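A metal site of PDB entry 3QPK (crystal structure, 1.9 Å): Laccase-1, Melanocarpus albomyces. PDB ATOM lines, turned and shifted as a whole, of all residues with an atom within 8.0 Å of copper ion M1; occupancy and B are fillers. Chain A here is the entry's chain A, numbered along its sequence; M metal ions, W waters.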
ATOM      1  N   HIS A  93     -22.856 -27.246 -30.469  1.00  0.00           N
ATOM      2  CA  HIS A  93     -22.413 -27.281 -29.089  1.00  0.00           C
ATOM      3  C   HIS A  93     -23.597 -27.074 -28.152  1.00  0.00           C
ATOM      4  O   HIS A  93     -24.476 -26.247 -28.397  1.00  0.00           O
ATOM      5  CB  HIS A  93     -21.287 -26.251 -28.869  1.00  0.00           C
ATOM      6  CG  HIS A  93     -20.913 -26.023 -27.443  1.00  0.00           C
ATOM      7  ND1 HIS A  93     -20.393 -27.017 -26.646  1.00  0.00           N
ATOM      8  CD2 HIS A  93     -20.958 -24.915 -26.661  1.00  0.00           C
ATOM      9  CE1 HIS A  93     -20.159 -26.547 -25.435  1.00  0.00           C
ATOM     10  NE2 HIS A  93     -20.495 -25.272 -25.418  1.00  0.00           N
ATOM     11  N   HIS A  95     -24.409 -25.695 -24.977  1.00  0.00           N
ATOM     12  CA  HIS A  95     -23.833 -24.750 -24.012  1.00  0.00           C
ATOM     13  C   HIS A  95     -24.414 -24.919 -22.610  1.00  0.00           C
ATOM     14  O   HIS A  95     -25.607 -24.687 -22.392  1.00  0.00           O
ATOM     15  CB  HIS A  95     -24.035 -23.317 -24.498  1.00  0.00           C
ATOM     16  CG  HIS A  95     -23.486 -22.276 -23.580  1.00  0.00           C
ATOM     17  ND1 HIS A  95     -22.601 -21.308 -24.005  1.00  0.00           N
ATOM     18  CD2 HIS A  95     -23.704 -22.040 -22.260  1.00  0.00           C
ATOM     19  CE1 HIS A  95     -22.290 -20.526 -22.973  1.00  0.00           C
ATOM     20  NE2 HIS A  95     -22.949 -20.951 -21.905  1.00  0.00           N
ATOM     21  N   ASP A 106     -19.517 -33.003 -27.542  1.00  0.00           N
ATOM     22  CA  ASP A 106     -19.481 -31.602 -27.116  1.00  0.00           C
ATOM     23  C   ASP A 106     -19.731 -30.593 -28.253  1.00  0.00           C
ATOM     24  O   ASP A 106     -20.138 -29.451 -28.011  1.00  0.00           O
ATOM     25  CB  ASP A 106     -18.148 -31.309 -26.397  1.00  0.00           C
ATOM     26  CG  ASP A 106     -18.060 -29.889 -25.860  1.00  0.00           C
ATOM     27  OD1 ASP A 106     -18.972 -29.445 -25.136  1.00  0.00           O
ATOM     28  OD2 ASP A 106     -17.058 -29.217 -26.144  1.00  0.00           O
ATOM     29  N   GLY A 107     -19.471 -30.997 -29.492  1.00  0.00           N
ATOM     30  CA  GLY A 107     -19.758 -30.146 -30.640  1.00  0.00           C
ATOM     31  C   GLY A 107     -18.718 -29.071 -30.958  1.00  0.00           C
ATOM     32  O   GLY A 107     -19.021 -28.113 -31.654  1.00  0.00           O
ATOM     33  N   ALA A 108     -17.508 -29.216 -30.443  1.00  0.00           N
ATOM     34  CA  ALA A 108     -16.439 -28.275 -30.780  1.00  0.00           C
ATOM     35  C   ALA A 108     -15.633 -28.746 -31.983  1.00  0.00           C
ATOM     36  O   ALA A 108     -14.627 -29.450 -31.833  1.00  0.00           O
ATOM     37  CB  ALA A 108     -15.523 -28.048 -29.582  1.00  0.00           C
ATOM     38  N   HIS A 138     -25.841 -24.177 -29.911  1.00  0.00           N
ATOM     39  CA  HIS A 138     -25.533 -23.335 -31.054  1.00  0.00           C
ATOM     40  C   HIS A 138     -24.411 -23.917 -31.865  1.00  0.00           C
ATOM     41  O   HIS A 138     -23.663 -24.745 -31.378  1.00  0.00           O
ATOM     42  CB  HIS A 138     -25.157 -21.924 -30.576  1.00  0.00           C
ATOM     43  CG  HIS A 138     -24.014 -21.897 -29.605  1.00  0.00           C
ATOM     44  ND1 HIS A 138     -22.698 -21.933 -30.008  1.00  0.00           N
ATOM     45  CD2 HIS A 138     -24.004 -21.821 -28.251  1.00  0.00           C
ATOM     46  CE1 HIS A 138     -21.916 -21.894 -28.939  1.00  0.00           C
ATOM     47  NE2 HIS A 138     -22.687 -21.831 -27.864  1.00  0.00           N
ATOM     48  N   SER A 139     -24.297 -23.505 -33.122  1.00  0.00           N
ATOM     49  CA  SER A 139     -23.167 -23.883 -33.948  1.00  0.00           C
ATOM     50  C   SER A 139     -21.862 -23.400 -33.355  1.00  0.00           C
ATOM     51  O   SER A 139     -21.787 -22.330 -32.724  1.00  0.00           O
ATOM     52  CB  SER A 139     -23.315 -23.327 -35.365  1.00  0.00           C
ATOM     53  OG  SER A 139     -22.151 -23.583 -36.131  1.00  0.00           O
ATOM     54  N   HIS A 140     -20.818 -24.205 -33.559  1.00  0.00           N
ATOM     55  CA  HIS A 140     -19.477 -23.798 -33.194  1.00  0.00           C
ATOM     56  C   HIS A 140     -18.617 -23.687 -34.455  1.00  0.00           C
ATOM     57  O   HIS A 140     -17.399 -23.715 -34.368  1.00  0.00           O
ATOM     58  CB  HIS A 140     -18.862 -24.749 -32.167  1.00  0.00           C
ATOM     59  CG  HIS A 140     -18.235 -24.035 -31.009  1.00  0.00           C
ATOM     60  ND1 HIS A 140     -17.115 -23.231 -31.146  1.00  0.00           N
ATOM     61  CD2 HIS A 140     -18.564 -23.990 -29.698  1.00  0.00           C
ATOM     62  CE1 HIS A 140     -16.790 -22.737 -29.962  1.00  0.00           C
ATOM     63  NE2 HIS A 140     -17.651 -23.181 -29.070  1.00  0.00           N
ATOM     64  N   TYR A 145     -23.386 -19.434 -35.771  1.00  0.00           N
ATOM     65  CA  TYR A 145     -24.609 -19.285 -34.982  1.00  0.00           C
ATOM     66  C   TYR A 145     -25.222 -17.880 -35.103  1.00  0.00           C
ATOM     67  O   TYR A 145     -26.409 -17.698 -34.855  1.00  0.00           O
ATOM     68  CB  TYR A 145     -24.438 -19.706 -33.511  1.00  0.00           C
ATOM     69  CG  TYR A 145     -23.885 -18.717 -32.476  1.00  0.00           C
ATOM     70  CD1 TYR A 145     -24.737 -17.872 -31.753  1.00  0.00           C
ATOM     71  CD2 TYR A 145     -22.543 -18.717 -32.131  1.00  0.00           C
ATOM     72  CE1 TYR A 145     -24.254 -17.013 -30.753  1.00  0.00           C
ATOM     73  CE2 TYR A 145     -22.037 -17.835 -31.145  1.00  0.00           C
ATOM     74  CZ  TYR A 145     -22.907 -17.000 -30.459  1.00  0.00           C
ATOM     75  OH  TYR A 145     -22.407 -16.149 -29.484  1.00  0.00           O
ATOM     76  N   HIS A 434     -16.001 -18.308 -21.049  1.00  0.00           N
ATOM     77  CA  HIS A 434     -16.860 -19.489 -20.979  1.00  0.00           C
ATOM     78  C   HIS A 434     -16.045 -20.765 -20.993  1.00  0.00           C
ATOM     79  O   HIS A 434     -15.161 -20.924 -21.835  1.00  0.00           O
ATOM     80  CB  HIS A 434     -17.864 -19.513 -22.147  1.00  0.00           C
ATOM     81  CG  HIS A 434     -18.630 -20.800 -22.250  1.00  0.00           C
ATOM     82  ND1 HIS A 434     -19.526 -21.218 -21.295  1.00  0.00           N
ATOM     83  CD2 HIS A 434     -18.612 -21.774 -23.200  1.00  0.00           C
ATOM     84  CE1 HIS A 434     -20.029 -22.383 -21.640  1.00  0.00           C
ATOM     85  NE2 HIS A 434     -19.487 -22.747 -22.795  1.00  0.00           N
ATOM     86  N   LEU A 435     -16.344 -21.677 -20.084  1.00  0.00           N
ATOM     87  CA  LEU A 435     -15.613 -22.943 -20.026  1.00  0.00           C
ATOM     88  C   LEU A 435     -16.503 -24.126 -20.415  1.00  0.00           C
ATOM     89  O   LEU A 435     -17.602 -24.288 -19.887  1.00  0.00           O
ATOM     90  CB  LEU A 435     -15.027 -23.168 -18.626  1.00  0.00           C
ATOM     91  CG  LEU A 435     -14.294 -24.484 -18.351  1.00  0.00           C
ATOM     92  CD1 LEU A 435     -13.101 -24.670 -19.269  1.00  0.00           C
ATOM     93  CD2 LEU A 435     -13.846 -24.531 -16.889  1.00  0.00           C
ATOM     94  N   HIS A 436     -16.015 -24.932 -21.367  1.00  0.00           N
ATOM     95  CA  HIS A 436     -16.714 -26.174 -21.749  1.00  0.00           C
ATOM     96  C   HIS A 436     -16.421 -27.238 -20.721  1.00  0.00           C
ATOM     97  O   HIS A 436     -15.344 -27.223 -20.111  1.00  0.00           O
ATOM     98  CB  HIS A 436     -16.195 -26.679 -23.096  1.00  0.00           C
ATOM     99  CG  HIS A 436     -16.617 -25.870 -24.285  1.00  0.00           C
ATOM    100  ND1 HIS A 436     -17.059 -26.436 -25.453  1.00  0.00           N
ATOM    101  CD2 HIS A 436     -16.671 -24.526 -24.477  1.00  0.00           C
ATOM    102  CE1 HIS A 436     -17.363 -25.486 -26.322  1.00  0.00           C
ATOM    103  NE2 HIS A 436     -17.142 -24.316 -25.750  1.00  0.00           N
ATOM    104  N   TRP A 499     -11.396 -29.542 -23.692  1.00  0.00           N
ATOM    105  CA  TRP A 499     -12.448 -28.584 -23.360  1.00  0.00           C
ATOM    106  C   TRP A 499     -12.053 -27.140 -23.656  1.00  0.00           C
ATOM    107  O   TRP A 499     -11.172 -26.603 -23.014  1.00  0.00           O
ATOM    108  CB  TRP A 499     -12.790 -28.682 -21.877  1.00  0.00           C
ATOM    109  CG  TRP A 499     -13.181 -30.045 -21.405  1.00  0.00           C
ATOM    110  CD1 TRP A 499     -12.485 -30.849 -20.547  1.00  0.00           C
ATOM    111  CD2 TRP A 499     -14.363 -30.763 -21.759  1.00  0.00           C
ATOM    112  NE1 TRP A 499     -13.153 -32.024 -20.343  1.00  0.00           N
ATOM    113  CE2 TRP A 499     -14.310 -32.000 -21.077  1.00  0.00           C
ATOM    114  CE3 TRP A 499     -15.448 -30.490 -22.600  1.00  0.00           C
ATOM    115  CZ2 TRP A 499     -15.316 -32.957 -21.205  1.00  0.00           C
ATOM    116  CZ3 TRP A 499     -16.449 -31.447 -22.720  1.00  0.00           C
ATOM    117  CH2 TRP A 499     -16.379 -32.666 -22.024  1.00  0.00           C
ATOM    118  N   LEU A 500     -12.741 -26.514 -24.595  1.00  0.00           N
ATOM    119  CA  LEU A 500     -12.432 -25.127 -24.945  1.00  0.00           C
ATOM    120  C   LEU A 500     -12.710 -24.167 -23.799  1.00  0.00           C
ATOM    121  O   LEU A 500     -13.633 -24.387 -23.007  1.00  0.00           O
ATOM    122  CB  LEU A 500     -13.238 -24.690 -26.183  1.00  0.00           C
ATOM    123  CG  LEU A 500     -12.797 -25.229 -27.550  1.00  0.00           C
ATOM    124  CD1 LEU A 500     -13.795 -24.828 -28.629  1.00  0.00           C
ATOM    125  CD2 LEU A 500     -11.367 -24.778 -27.887  1.00  0.00           C
ATOM    126  N   PHE A 501     -11.908 -23.109 -23.714  1.00  0.00           N
ATOM    127  CA  PHE A 501     -12.123 -22.031 -22.763  1.00  0.00           C
ATOM    128  C   PHE A 501     -11.814 -20.726 -23.477  1.00  0.00           C
ATOM    129  O   PHE A 501     -10.666 -20.478 -23.873  1.00  0.00           O
ATOM    130  CB  PHE A 501     -11.239 -22.188 -21.535  1.00  0.00           C
ATOM    131  CG  PHE A 501     -11.321 -21.040 -20.576  1.00  0.00           C
ATOM    132  CD1 PHE A 501     -12.521 -20.672 -19.997  1.00  0.00           C
ATOM    133  CD2 PHE A 501     -10.164 -20.356 -20.207  1.00  0.00           C
ATOM    134  CE1 PHE A 501     -12.581 -19.618 -19.086  1.00  0.00           C
ATOM    135  CE2 PHE A 501     -10.216 -19.305 -19.302  1.00  0.00           C
ATOM    136  CZ  PHE A 501     -11.428 -18.935 -18.739  1.00  0.00           C
ATOM    137  N   HIS A 502     -12.835 -19.904 -23.633  1.00  0.00           N
ATOM    138  CA  HIS A 502     -12.735 -18.798 -24.569  1.00  0.00           C
ATOM    139  C   HIS A 502     -13.718 -17.676 -24.274  1.00  0.00           C
ATOM    140  O   HIS A 502     -14.668 -17.852 -23.521  1.00  0.00           O
ATOM    141  CB  HIS A 502     -12.948 -19.327 -25.985  1.00  0.00           C
ATOM    142  CG  HIS A 502     -14.332 -19.835 -26.240  1.00  0.00           C
ATOM    143  ND1 HIS A 502     -15.349 -19.039 -26.709  1.00  0.00           N
ATOM    144  CD2 HIS A 502     -14.863 -21.073 -26.101  1.00  0.00           C
ATOM    145  CE1 HIS A 502     -16.457 -19.751 -26.844  1.00  0.00           C
ATOM    146  NE2 HIS A 502     -16.195 -20.997 -26.486  1.00  0.00           N
ATOM    147  N   CYS A 503     -13.443 -16.502 -24.850  1.00  0.00           N
ATOM    148  CA  CYS A 503     -14.419 -15.415 -24.858  1.00  0.00           C
ATOM    149  C   CYS A 503     -15.599 -15.840 -25.746  1.00  0.00           C
ATOM    150  O   CYS A 503     -15.391 -16.449 -26.803  1.00  0.00           O
ATOM    151  CB  CYS A 503     -13.805 -14.142 -25.423  1.00  0.00           C
ATOM    152  SG  CYS A 503     -15.030 -12.870 -25.559  1.00  0.00           S
ATOM    153  N   HIS A 504     -16.815 -15.526 -25.319  1.00  0.00           N
ATOM    154  CA  HIS A 504     -18.004 -15.954 -26.078  1.00  0.00           C
ATOM    155  C   HIS A 504     -18.522 -14.922 -27.083  1.00  0.00           C
ATOM    156  O   HIS A 504     -19.566 -15.145 -27.707  1.00  0.00           O
ATOM    157  CB  HIS A 504     -19.149 -16.350 -25.140  1.00  0.00           C
ATOM    158  CG  HIS A 504     -20.057 -17.404 -25.716  1.00  0.00           C
ATOM    159  ND1 HIS A 504     -20.930 -17.155 -26.748  1.00  0.00           N
ATOM    160  CD2 HIS A 504     -20.208 -18.711 -25.399  1.00  0.00           C
ATOM    161  CE1 HIS A 504     -21.583 -18.265 -27.042  1.00  0.00           C
ATOM    162  NE2 HIS A 504     -21.151 -19.224 -26.241  1.00  0.00           N
ATOM    163  N   VAL A 509     -13.470 -14.898 -30.193  1.00  0.00           N
ATOM    164  CA  VAL A 509     -13.041 -16.286 -30.346  1.00  0.00           C
ATOM    165  C   VAL A 509     -12.675 -16.535 -31.809  1.00  0.00           C
ATOM    166  O   VAL A 509     -11.721 -17.255 -32.104  1.00  0.00           O
ATOM    167  CB  VAL A 509     -14.065 -17.339 -29.791  1.00  0.00           C
ATOM    168  CG1 VAL A 509     -15.348 -17.362 -30.587  1.00  0.00           C
ATOM    169  CG2 VAL A 509     -13.427 -18.754 -29.702  1.00  0.00           C
ATOM    170  N   SER A 514      -8.982 -17.970 -27.157  1.00  0.00           N
ATOM    171  CA  SER A 514      -9.377 -19.235 -26.563  1.00  0.00           C
ATOM    172  C   SER A 514      -8.175 -20.078 -26.169  1.00  0.00           C
ATOM    173  O   SER A 514      -7.094 -19.925 -26.734  1.00  0.00           O
ATOM    174  CB  SER A 514     -10.254 -20.030 -27.548  1.00  0.00           C
ATOM    175  OG  SER A 514     -10.635 -21.286 -27.025  1.00  0.00           O
ATOM    176  N   LEU A 559     -13.557 -21.315 -34.781  1.00  0.00           N
ATOM    177  CA  LEU A 559     -14.402 -21.438 -33.581  1.00  0.00           C
ATOM    178  C   LEU A 559     -15.338 -20.257 -33.389  1.00  0.00           C
ATOM    179  O   LEU A 559     -16.218 -20.315 -32.529  1.00  0.00           O
ATOM    180  CB  LEU A 559     -13.524 -21.551 -32.345  1.00  0.00           C
ATOM    181  CG  LEU A 559     -12.667 -22.819 -32.291  1.00  0.00           C
ATOM    182  CD1 LEU A 559     -11.844 -22.850 -31.010  1.00  0.00           C
ATOM    183  CD2 LEU A 559     -13.579 -24.049 -32.408  1.00  0.00           C
ATOM    184  OXT LEU A 559     -15.208 -19.220 -34.044  1.00  0.00           O
HETATM  185 CU    CU M   1     -17.446 -22.715 -27.026  1.00  0.00          CU
HETATM  186 CU    CU M   2     -20.049 -23.972 -24.185  1.00  0.00          CU
HETATM  187 CU    CU M   3     -22.032 -21.084 -26.059  1.00  0.00          CU
HETATM  188  O   HOH W   1     -19.654 -21.942 -26.582  1.00  0.00           O
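N of His 436 is in hydrogen-bond range of O of Leu 500 (2.9 Å). OD2 of Asp 106 is in hydrogen-bond range of ND1 of His 436 (2.9 Å). O of Leu 559 lies within hydrogen-bond range of ND1 of His 140, at 3.3 Å. O of His 502 is in hydrogen-bond range of N of His 434.
Copper ion M1 is bound by NE2 of His 436 (2.1 Å). Copper ion M1 is bound by NE2 of His 140 (2.1 Å). Copper ion M1 is bound by NE2 of His 502 (2.2 Å). Copper ion M1 is bound by water W1, at 2.4 Å. Copper ion M1 has four donor atoms within binding distance.
Three residues have an atom within 4 Å of copper ion M1: His 140, His 436 and His 502. Along chain A the residues within 4 Å of copper ion M1 span positions 140 to 502.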
